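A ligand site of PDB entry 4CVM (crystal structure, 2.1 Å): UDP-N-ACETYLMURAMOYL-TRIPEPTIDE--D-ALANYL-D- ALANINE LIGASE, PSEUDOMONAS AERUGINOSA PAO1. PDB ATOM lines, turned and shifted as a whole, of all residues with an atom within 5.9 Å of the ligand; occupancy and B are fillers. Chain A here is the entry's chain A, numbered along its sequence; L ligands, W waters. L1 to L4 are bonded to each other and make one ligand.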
ATOM      1  N   THR A  30      23.128 -14.497 -14.682  1.00  0.00           N
ATOM      2  CA  THR A  30      24.453 -14.896 -14.214  1.00  0.00           C
ATOM      3  C   THR A  30      25.400 -15.056 -15.348  1.00  0.00           C
ATOM      4  O   THR A  30      26.481 -15.593 -15.139  1.00  0.00           O
ATOM      5  CB  THR A  30      24.427 -16.220 -13.451  1.00  0.00           C
ATOM      6  OG1 THR A  30      23.833 -17.204 -14.274  1.00  0.00           O
ATOM      7  CG2 THR A  30      23.589 -16.024 -12.169  1.00  0.00           C
ATOM      8  N   ASP A  31      25.056 -14.525 -16.525  1.00  0.00           N
ATOM      9  CA  ASP A  31      25.875 -14.775 -17.709  1.00  0.00           C
ATOM     10  C   ASP A  31      25.949 -13.570 -18.643  1.00  0.00           C
ATOM     11  O   ASP A  31      24.955 -13.140 -19.218  1.00  0.00           O
ATOM     12  CB  ASP A  31      25.339 -16.037 -18.441  1.00  0.00           C
ATOM     13  CG  ASP A  31      26.359 -16.618 -19.388  1.00  0.00           C
ATOM     14  OD1 ASP A  31      27.197 -15.855 -19.962  1.00  0.00           O
ATOM     15  OD2 ASP A  31      26.350 -17.853 -19.523  1.00  0.00           O
ATOM     16  N   SER A  32      27.132 -13.005 -18.819  1.00  0.00           N
ATOM     17  CA  SER A  32      27.292 -11.857 -19.736  1.00  0.00           C
ATOM     18  C   SER A  32      26.914 -12.152 -21.159  1.00  0.00           C
ATOM     19  O   SER A  32      26.568 -11.223 -21.885  1.00  0.00           O
ATOM     20  CB  SER A  32      28.727 -11.321 -19.761  1.00  0.00           C
ATOM     21  OG  SER A  32      29.552 -12.267 -20.335  1.00  0.00           O
ATOM     22  N   ARG A  33      26.942 -13.430 -21.530  1.00  0.00           N
ATOM     23  CA  ARG A  33      26.496 -13.849 -22.875  1.00  0.00           C
ATOM     24  C   ARG A  33      24.995 -13.849 -23.022  1.00  0.00           C
ATOM     25  O   ARG A  33      24.544 -13.986 -24.132  1.00  0.00           O
ATOM     26  CB  ARG A  33      27.033 -15.240 -23.208  1.00  0.00           C
ATOM     27  CG  ARG A  33      28.543 -15.238 -23.218  1.00  0.00           C
ATOM     28  CD  ARG A  33      29.159 -16.634 -23.126  1.00  0.00           C
ATOM     29  NE  ARG A  33      28.815 -17.304 -21.877  1.00  0.00           N
ATOM     30  CZ  ARG A  33      29.438 -18.371 -21.381  1.00  0.00           C
ATOM     31  NH1 ARG A  33      30.485 -18.902 -22.001  1.00  0.00           N
ATOM     32  NH2 ARG A  33      29.010 -18.935 -20.262  1.00  0.00           N
ATOM     33  N   PHE A  41      23.275  -8.138 -13.220  1.00  0.00           N
ATOM     34  CA  PHE A  41      24.271  -9.171 -13.474  1.00  0.00           C
ATOM     35  C   PHE A  41      24.783  -9.713 -12.109  1.00  0.00           C
ATOM     36  O   PHE A  41      25.057  -8.943 -11.168  1.00  0.00           O
ATOM     37  CB  PHE A  41      25.451  -8.650 -14.239  1.00  0.00           C
ATOM     38  CG  PHE A  41      26.511  -9.652 -14.479  1.00  0.00           C
ATOM     39  CD1 PHE A  41      26.259 -10.794 -15.221  1.00  0.00           C
ATOM     40  CD2 PHE A  41      27.820  -9.413 -14.065  1.00  0.00           C
ATOM     41  CE1 PHE A  41      27.280 -11.702 -15.490  1.00  0.00           C
ATOM     42  CE2 PHE A  41      28.835 -10.288 -14.376  1.00  0.00           C
ATOM     43  CZ  PHE A  41      28.569 -11.445 -15.057  1.00  0.00           C
ATOM     44  N   ILE A  42      24.890 -11.015 -12.032  1.00  0.00           N
ATOM     45  CA  ILE A  42      25.407 -11.666 -10.886  1.00  0.00           C
ATOM     46  C   ILE A  42      26.728 -12.342 -11.252  1.00  0.00           C
ATOM     47  O   ILE A  42      26.765 -13.212 -12.077  1.00  0.00           O
ATOM     48  CB  ILE A  42      24.418 -12.655 -10.302  1.00  0.00           C
ATOM     49  CG1 ILE A  42      23.183 -11.890  -9.857  1.00  0.00           C
ATOM     50  CG2 ILE A  42      25.002 -13.269  -9.034  1.00  0.00           C
ATOM     51  CD1 ILE A  42      22.140 -12.706  -9.133  1.00  0.00           C
ATOM     52  N   LEU A  44      29.550 -14.794 -10.652  1.00  0.00           N
ATOM     53  CA  LEU A  44      29.947 -16.044 -10.049  1.00  0.00           C
ATOM     54  C   LEU A  44      31.305 -16.504 -10.537  1.00  0.00           C
ATOM     55  O   LEU A  44      31.675 -16.286 -11.697  1.00  0.00           O
ATOM     56  CB  LEU A  44      28.948 -17.152 -10.412  1.00  0.00           C
ATOM     57  CG  LEU A  44      27.471 -16.851 -10.107  1.00  0.00           C
ATOM     58  CD1 LEU A  44      26.598 -17.835 -10.838  1.00  0.00           C
ATOM     59  CD2 LEU A  44      27.192 -16.896  -8.620  1.00  0.00           C
ATOM     60  N   SER A  45      32.044 -17.161  -9.644  1.00  0.00           N
ATOM     61  CA  SER A  45      33.295 -17.865 -10.000  1.00  0.00           C
ATOM     62  C   SER A  45      33.065 -19.330 -10.282  1.00  0.00           C
ATOM     63  O   SER A  45      32.270 -19.970  -9.632  1.00  0.00           O
ATOM     64  CB  SER A  45      34.304 -17.754  -8.856  1.00  0.00           C
ATOM     65  OG  SER A  45      35.031 -16.549  -9.009  1.00  0.00           O
ATOM     66  N   GLY A  46      33.741 -19.852 -11.285  1.00  0.00           N
ATOM     67  CA  GLY A  46      33.623 -21.233 -11.620  1.00  0.00           C
ATOM     68  C   GLY A  46      34.972 -21.843 -11.924  1.00  0.00           C
ATOM     69  O   GLY A  46      36.025 -21.202 -11.736  1.00  0.00           O
ATOM     70  N   PRO A  47      34.949 -23.068 -12.427  1.00  0.00           N
ATOM     71  CA  PRO A  47      36.193 -23.778 -12.780  1.00  0.00           C
ATOM     72  C   PRO A  47      36.875 -23.237 -14.057  1.00  0.00           C
ATOM     73  O   PRO A  47      38.082 -23.391 -14.189  1.00  0.00           O
ATOM     74  CB  PRO A  47      35.732 -25.212 -12.959  1.00  0.00           C
ATOM     75  CG  PRO A  47      34.231 -25.125 -13.273  1.00  0.00           C
ATOM     76  CD  PRO A  47      33.742 -23.899 -12.606  1.00  0.00           C
ATOM     77  N   ARG A  48      36.113 -22.606 -14.960  1.00  0.00           N
ATOM     78  CA  ARG A  48      36.615 -22.105 -16.243  1.00  0.00           C
ATOM     79  C   ARG A  48      36.669 -20.584 -16.322  1.00  0.00           C
ATOM     80  O   ARG A  48      37.637 -20.023 -16.839  1.00  0.00           O
ATOM     81  CB  ARG A  48      35.801 -22.707 -17.395  1.00  0.00           C
ATOM     82  N   PHE A  49      35.670 -19.879 -15.783  1.00  0.00           N
ATOM     83  CA  PHE A  49      35.647 -18.414 -15.859  1.00  0.00           C
ATOM     84  C   PHE A  49      35.340 -17.735 -14.533  1.00  0.00           C
ATOM     85  O   PHE A  49      34.854 -18.341 -13.584  1.00  0.00           O
ATOM     86  CB  PHE A  49      34.604 -17.963 -16.883  1.00  0.00           C
ATOM     87  CG  PHE A  49      34.755 -18.588 -18.260  1.00  0.00           C
ATOM     88  CD1 PHE A  49      35.742 -18.162 -19.134  1.00  0.00           C
ATOM     89  CD2 PHE A  49      33.867 -19.556 -18.699  1.00  0.00           C
ATOM     90  CE1 PHE A  49      35.858 -18.712 -20.420  1.00  0.00           C
ATOM     91  CE2 PHE A  49      33.964 -20.116 -19.956  1.00  0.00           C
ATOM     92  CZ  PHE A  49      34.966 -19.706 -20.824  1.00  0.00           C
ATOM     93  N   ASP A  50      35.581 -16.453 -14.503  1.00  0.00           N
ATOM     94  CA  ASP A  50      35.157 -15.620 -13.382  1.00  0.00           C
ATOM     95  C   ASP A  50      34.229 -14.485 -13.864  1.00  0.00           C
ATOM     96  O   ASP A  50      34.648 -13.579 -14.616  1.00  0.00           O
ATOM     97  CB  ASP A  50      36.373 -15.014 -12.674  1.00  0.00           C
ATOM     98  CG  ASP A  50      35.988 -14.254 -11.426  1.00  0.00           C
ATOM     99  OD1 ASP A  50      34.778 -14.087 -11.127  1.00  0.00           O
ATOM    100  OD2 ASP A  50      36.899 -13.809 -10.708  1.00  0.00           O
ATOM    101  N   GLY A  51      32.973 -14.509 -13.419  1.00  0.00           N
ATOM    102  CA  GLY A  51      32.036 -13.451 -13.795  1.00  0.00           C
ATOM    103  C   GLY A  51      32.491 -12.006 -13.581  1.00  0.00           C
ATOM    104  O   GLY A  51      32.062 -11.061 -14.304  1.00  0.00           O
ATOM    105  N   TYR A  54      33.708  -9.549 -16.426  1.00  0.00           N
ATOM    106  CA  TYR A  54      32.816  -9.172 -17.560  1.00  0.00           C
ATOM    107  C   TYR A  54      31.989  -7.914 -17.312  1.00  0.00           C
ATOM    108  O   TYR A  54      30.925  -7.724 -17.936  1.00  0.00           O
ATOM    109  CB  TYR A  54      31.907 -10.356 -17.962  1.00  0.00           C
ATOM    110  CG  TYR A  54      32.745 -11.520 -18.371  1.00  0.00           C
ATOM    111  CD1 TYR A  54      33.294 -11.602 -19.669  1.00  0.00           C
ATOM    112  CD2 TYR A  54      33.067 -12.519 -17.467  1.00  0.00           C
ATOM    113  CE1 TYR A  54      34.115 -12.659 -20.008  1.00  0.00           C
ATOM    114  CE2 TYR A  54      33.879 -13.568 -17.813  1.00  0.00           C
ATOM    115  CZ  TYR A  54      34.405 -13.638 -19.079  1.00  0.00           C
ATOM    116  OH  TYR A  54      35.254 -14.690 -19.409  1.00  0.00           O
ATOM    117  N   ARG A  86      26.770 -16.556  -4.634  1.00  0.00           N
ATOM    118  CA  ARG A  86      25.914 -17.761  -4.664  1.00  0.00           C
ATOM    119  C   ARG A  86      24.851 -17.665  -3.596  1.00  0.00           C
ATOM    120  O   ARG A  86      23.675 -17.817  -3.896  1.00  0.00           O
ATOM    121  CB  ARG A  86      26.671 -19.065  -4.495  1.00  0.00           C
ATOM    122  CG  ARG A  86      27.720 -19.237  -5.555  1.00  0.00           C
ATOM    123  CD  ARG A  86      28.475 -20.531  -5.429  1.00  0.00           C
ATOM    124  NE  ARG A  86      29.189 -20.756  -6.698  1.00  0.00           N
ATOM    125  CZ  ARG A  86      28.868 -21.668  -7.614  1.00  0.00           C
ATOM    126  NH1 ARG A  86      27.851 -22.534  -7.427  1.00  0.00           N
ATOM    127  NH2 ARG A  86      29.597 -21.734  -8.740  1.00  0.00           N
ATOM    128  N   GLY A 139      14.687 -26.579 -18.588  1.00  0.00           N
ATOM    129  CA  GLY A 139      15.696 -27.661 -18.726  1.00  0.00           C
ATOM    130  C   GLY A 139      15.904 -28.391 -17.427  1.00  0.00           C
ATOM    131  O   GLY A 139      14.948 -28.891 -16.741  1.00  0.00           O
ATOM    132  N   ASN A 140      17.163 -28.389 -17.017  1.00  0.00           N
ATOM    133  CA  ASN A 140      17.542 -29.015 -15.821  1.00  0.00           C
ATOM    134  C   ASN A 140      18.128 -28.077 -14.773  1.00  0.00           C
ATOM    135  O   ASN A 140      19.013 -28.480 -13.997  1.00  0.00           O
ATOM    136  CB  ASN A 140      18.529 -30.070 -16.191  1.00  0.00           C
ATOM    137  CG  ASN A 140      18.301 -31.317 -15.449  1.00  0.00           C
ATOM    138  OD1 ASN A 140      17.152 -31.800 -15.378  1.00  0.00           O
ATOM    139  ND2 ASN A 140      19.365 -31.846 -14.881  1.00  0.00           N
ATOM    140  N   LEU A 141      17.620 -26.852 -14.711  1.00  0.00           N
ATOM    141  CA  LEU A 141      18.149 -25.812 -13.805  1.00  0.00           C
ATOM    142  C   LEU A 141      17.681 -26.106 -12.369  1.00  0.00           C
ATOM    143  O   LEU A 141      16.748 -25.482 -11.868  1.00  0.00           O
ATOM    144  CB  LEU A 141      17.698 -24.409 -14.246  1.00  0.00           C
ATOM    145  CG  LEU A 141      18.313 -23.893 -15.558  1.00  0.00           C
ATOM    146  CD1 LEU A 141      17.894 -22.460 -15.849  1.00  0.00           C
ATOM    147  CD2 LEU A 141      19.817 -23.966 -15.629  1.00  0.00           C
ATOM    148  N   ASN A 142      18.341 -27.065 -11.717  1.00  0.00           N
ATOM    149  CA  ASN A 142      17.802 -27.631 -10.482  1.00  0.00           C
ATOM    150  C   ASN A 142      18.726 -27.663  -9.273  1.00  0.00           C
ATOM    151  O   ASN A 142      18.355 -28.262  -8.244  1.00  0.00           O
ATOM    152  CB  ASN A 142      17.249 -29.041 -10.751  1.00  0.00           C
ATOM    153  CG  ASN A 142      18.332 -30.078 -11.034  1.00  0.00           C
ATOM    154  OD1 ASN A 142      19.486 -29.856 -10.770  1.00  0.00           O
ATOM    155  ND2 ASN A 142      17.928 -31.228 -11.521  1.00  0.00           N
ATOM    156  N   ASN A 143      19.888 -27.004  -9.354  1.00  0.00           N
ATOM    157  CA  ASN A 143      20.881 -27.111  -8.284  1.00  0.00           C
ATOM    158  C   ASN A 143      20.864 -25.849  -7.446  1.00  0.00           C
ATOM    159  O   ASN A 143      19.902 -25.051  -7.519  1.00  0.00           O
ATOM    160  CB  ASN A 143      22.299 -27.496  -8.834  1.00  0.00           C
ATOM    161  CG  ASN A 143      22.966 -26.364  -9.660  1.00  0.00           C
ATOM    162  OD1 ASN A 143      22.505 -25.215  -9.695  1.00  0.00           O
ATOM    163  ND2 ASN A 143      24.074 -26.696 -10.292  1.00  0.00           N
ATOM    164  N   ASP A 144      21.894 -25.631  -6.654  1.00  0.00           N
ATOM    165  CA  ASP A 144      21.878 -24.503  -5.791  1.00  0.00           C
ATOM    166  C   ASP A 144      21.916 -23.157  -6.516  1.00  0.00           C
ATOM    167  O   ASP A 144      21.637 -22.176  -5.881  1.00  0.00           O
ATOM    168  CB  ASP A 144      22.941 -24.608  -4.687  1.00  0.00           C
ATOM    169  CG  ASP A 144      24.353 -24.571  -5.224  1.00  0.00           C
ATOM    170  OD1 ASP A 144      24.593 -24.903  -6.387  1.00  0.00           O
ATOM    171  OD2 ASP A 144      25.245 -24.267  -4.417  1.00  0.00           O
ATOM    172  N   LEU A 145      22.198 -23.126  -7.817  1.00  0.00           N
ATOM    173  CA  LEU A 145      22.041 -21.890  -8.649  1.00  0.00           C
ATOM    174  C   LEU A 145      20.758 -21.941  -9.463  1.00  0.00           C
ATOM    175  O   LEU A 145      20.033 -20.887  -9.606  1.00  0.00           O
ATOM    176  CB  LEU A 145      23.213 -21.735  -9.653  1.00  0.00           C
ATOM    177  CG  LEU A 145      24.655 -21.834  -9.103  1.00  0.00           C
ATOM    178  CD1 LEU A 145      25.701 -21.694 -10.192  1.00  0.00           C
ATOM    179  CD2 LEU A 145      24.874 -20.806  -8.013  1.00  0.00           C
ATOM    180  N   GLY A 146      20.478 -23.111 -10.050  1.00  0.00           N
ATOM    181  CA  GLY A 146      19.329 -23.293 -10.910  1.00  0.00           C
ATOM    182  C   GLY A 146      18.013 -22.964 -10.217  1.00  0.00           C
ATOM    183  O   GLY A 146      17.104 -22.328 -10.770  1.00  0.00           O
ATOM    184  N   VAL A 147      17.850 -23.455  -9.000  1.00  0.00           N
ATOM    185  CA  VAL A 147      16.592 -23.214  -8.254  1.00  0.00           C
ATOM    186  C   VAL A 147      16.302 -21.745  -7.969  1.00  0.00           C
ATOM    187  O   VAL A 147      15.228 -21.290  -8.310  1.00  0.00           O
ATOM    188  CB  VAL A 147      16.544 -24.020  -6.981  1.00  0.00           C
ATOM    189  CG1 VAL A 147      15.289 -23.684  -6.206  1.00  0.00           C
ATOM    190  CG2 VAL A 147      16.594 -25.496  -7.312  1.00  0.00           C
ATOM    191  N   LEU A 149      17.431 -19.183  -9.625  1.00  0.00           N
ATOM    192  CA  LEU A 149      17.202 -18.597 -10.965  1.00  0.00           C
ATOM    193  C   LEU A 149      15.780 -18.878 -11.425  1.00  0.00           C
ATOM    194  O   LEU A 149      15.113 -18.012 -11.995  1.00  0.00           O
ATOM    195  CB  LEU A 149      18.202 -19.098 -12.015  1.00  0.00           C
ATOM    196  CG  LEU A 149      19.630 -18.525 -11.840  1.00  0.00           C
ATOM    197  CD1 LEU A 149      20.605 -19.215 -12.786  1.00  0.00           C
ATOM    198  CD2 LEU A 149      19.631 -17.013 -12.016  1.00  0.00           C
HETATM  199  N1  LIG L   1      30.541 -16.081 -17.555  1.00  0.00           N
HETATM  200  C1  LIG L   1      30.169 -14.871 -18.092  1.00  0.00           C
HETATM  201  N2  LIG L   1      30.595 -14.515 -19.325  1.00  0.00           N
HETATM  202  C2  LIG L   1      31.457 -15.349 -20.062  1.00  0.00           C
HETATM  203  C3  LIG L   1      31.870 -16.556 -19.522  1.00  0.00           C
HETATM  204  C4  LIG L   1      31.385 -16.933 -18.273  1.00  0.00           C
HETATM  205  O1  LIG L   1      29.437 -14.104 -17.499  1.00  0.00           O
HETATM  206  O2  LIG L   1      31.832 -14.987 -21.184  1.00  0.00           O
HETATM  207  C5  LIG L   1      30.083 -16.512 -16.229  1.00  0.00           C
HETATM  208  C6  LIG L   1      29.261 -17.778 -16.360  1.00  0.00           C
HETATM  209  O3  LIG L   1      27.918 -17.544 -16.783  1.00  0.00           O
HETATM  210  C7  LIG L   1      29.333 -18.302 -14.973  1.00  0.00           C
HETATM  211  C8  LIG L   1      30.731 -17.753 -14.488  1.00  0.00           C
HETATM  212  O4  LIG L   1      31.241 -17.015 -15.562  1.00  0.00           O
HETATM  213  O5  LIG L   1      28.337 -17.760 -14.135  1.00  0.00           O
HETATM  214  C9  LIG L   1      31.668 -18.955 -14.228  1.00  0.00           C
HETATM  215  O6  LIG L   1      31.705 -19.676 -15.430  1.00  0.00           O
HETATM  216  P1  LIG L   1      32.107 -21.214 -15.337  1.00  0.00           P
HETATM  217  O7  LIG L   1      33.563 -21.195 -14.808  1.00  0.00           O
HETATM  218  O8  LIG L   1      31.268 -21.949 -14.302  1.00  0.00           O
HETATM  219  O9  LIG L   1      32.128 -21.848 -16.743  1.00  0.00           O
HETATM  220  P2  LIG L   1      31.037 -21.840 -17.931  1.00  0.00           P
HETATM  221  O10 LIG L   1      30.624 -20.420 -18.378  1.00  0.00           O
HETATM  222  O11 LIG L   1      31.373 -22.663 -19.045  1.00  0.00           O
HETATM  223  C1  LG2 L   2      28.372 -21.718 -17.262  1.00  0.00           C
HETATM  224  C2  LG2 L   2      27.484 -22.246 -16.101  1.00  0.00           C
HETATM  225  C3  LG2 L   2      27.246 -23.713 -16.314  1.00  0.00           C
HETATM  226  C4  LG2 L   2      26.684 -23.859 -17.702  1.00  0.00           C
HETATM  227  C5  LG2 L   2      27.717 -23.326 -18.698  1.00  0.00           C
HETATM  228  C6  LG2 L   2      27.273 -23.649 -20.101  1.00  0.00           C
HETATM  229  C7  LG2 L   2      27.559 -21.418 -13.789  1.00  0.00           C
HETATM  230  C8  LG2 L   2      28.410 -21.114 -12.568  1.00  0.00           C
HETATM  231  C9  LG2 L   2      26.706 -24.857 -14.239  1.00  0.00           C
HETATM  232  C10 LG2 L   2      25.499 -24.817 -13.247  1.00  0.00           C
HETATM  233  C11 LG2 L   2      27.194 -26.300 -14.472  1.00  0.00           C
HETATM  234  O1  LG2 L   2      29.611 -22.466 -17.282  1.00  0.00           O
HETATM  235  O2  LG2 L   2      26.265 -24.299 -15.483  1.00  0.00           O
HETATM  236  O3  LG2 L   2      26.465 -25.188 -17.949  1.00  0.00           O
HETATM  237  O4  LG2 L   2      27.789 -21.903 -18.530  1.00  0.00           O
HETATM  238  O5  LG2 L   2      26.208 -22.766 -20.327  1.00  0.00           O
HETATM  239  O6  LG2 L   2      26.337 -21.381 -13.723  1.00  0.00           O
HETATM  240  O7  LG2 L   2      25.593 -25.196 -12.083  1.00  0.00           O
HETATM  241  N1  LG2 L   2      28.206 -21.942 -14.855  1.00  0.00           N
HETATM  242  N1  LG3 L   3      24.389 -24.322 -13.771  1.00  0.00           N
HETATM  243  C1  LG3 L   3      23.157 -24.193 -12.968  1.00  0.00           C
HETATM  244  C2  LG3 L   3      22.269 -25.484 -13.135  1.00  0.00           C
HETATM  245  O1  LG3 L   3      21.288 -25.685 -12.403  1.00  0.00           O
HETATM  246  C3  LG3 L   3      22.473 -22.879 -13.378  1.00  0.00           C
HETATM  247  N1  LG4 L   4      22.729 -26.502 -13.927  1.00  0.00           N
HETATM  248  C1  LG4 L   4      21.932 -27.730 -13.994  1.00  0.00           C
HETATM  249  C2  LG4 L   4      22.101 -28.356 -15.368  1.00  0.00           C
HETATM  250  O1  LG4 L   4      23.035 -29.138 -15.502  1.00  0.00           O
HETATM  251  C3  LG4 L   4      22.272 -28.751 -12.888  1.00  0.00           C
HETATM  252  O2  LG4 L   4      21.311 -27.973 -16.274  1.00  0.00           O
HETATM  253  O   HOH W   1      25.653 -19.474 -17.375  1.00  0.00           O
HETATM  254  O   HOH W   2      30.877 -22.007 -21.441  1.00  0.00           O
HETATM  255  O   HOH W   3      25.795 -18.891 -14.802  1.00  0.00           O
HETATM  256  O   HOH W   4      28.766 -14.793 -13.426  1.00  0.00           O
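The backbone NH (N) of Phe 49 is in hydrogen-bond range of an oxygen (O7) of LIG L1, 2.7 Å away.
ND2 of Asn 143 sits at hydrogen-bond distance from O7 of LG2 L2, 2.8 Å away.
N of Ser 32 sits at hydrogen-bond distance from O1 of LIG L1.
The backbone NH of Asn 142 sits at hydrogen-bond distance from an oxygen (O1) of LG3 L3, at 3.3 Å.
OG of Ser 32 is in hydrogen-bond range of N2 of LIG L1, at 2.7 Å.
O3 of LIG L1 lies within hydrogen-bond range of O of Thr 30 (2.9 Å).
O3 of LIG L1 is in hydrogen-bond range of OD2 of Asp 31, at 3.2 Å.
An oxygen (O10) of LIG L1 lies within salt-bridge range of the guanidinium group (NH2) of Arg 33 (2.9 Å).
An oxygen (O7) of LIG L1 lies within hydrogen-bond range of the backbone NH (N) of Arg 48.
NE of Arg 33 lies within salt-bridge range of OD1 of Asp 31.
O of Leu 44 sits at hydrogen-bond distance from N of Gly 51, at 2.8 Å.
N of Gly 146 sits at hydrogen-bond distance from OD1 of Asn 143.
The side-chain amide oxygen (OD1) of Asn 143 sits at hydrogen-bond distance from the backbone NH (N) of Leu 145 (2.8 Å).
An oxygen (O7) of LIG L1 sits close to the backbone nitrogen (N) of Pro 47 (3.3 Å).
O of Asn 140 sits close to O2 of LG4 L4, at 3.3 Å.
Residues that only touch the ligand: Gly 46 (3.2 Å), Leu 44 (3.3 Å), Gly 146 (3.4 Å), Leu 141 (3.4 Å), Tyr 54 (3.5 Å), Leu 145 (3.6 Å), Phe 41 (3.7 Å) and Gly 51 (3.7 Å).
Hydrophobic or aromatic side chains that line the ligand: Phe 41, Leu 44, Pro 47, Phe 49, Tyr 54, Leu 141 and Leu 145.
Within 4 Å of the ligand: Thr 30, Asp 31, Ser 32, Arg 33, Phe 41, Leu 44, Gly 46, Pro 47, Arg 48, Phe 49, Gly 51, Tyr 54, Asn 140, Leu 141, Asn 142, Asn 143, Leu 145 and Gly 146.
Water W2 bridges an oxygen (O11) of LIG L1 and the guanidinium group (NH1) of Arg 33.
Water W3 lies within hydrogen-bond range of OG1 of Thr 30 and O6 of LG2 L2.
Water W1 lies within hydrogen-bond range of the side-chain carboxylate of Asp 31 (2.8 Å) and an oxygen (O3) of LIG L1 (3.0 Å).
Water W4 lies within hydrogen-bond range of the backbone NH of Leu 44 (2.9 Å), the backbone carbonyl oxygen of Ile 42 (2.9 Å), the backbone carbonyl oxygen of Thr 30 (3.0 Å) and an oxygen (O5) of LIG L1 (3.1 Å).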
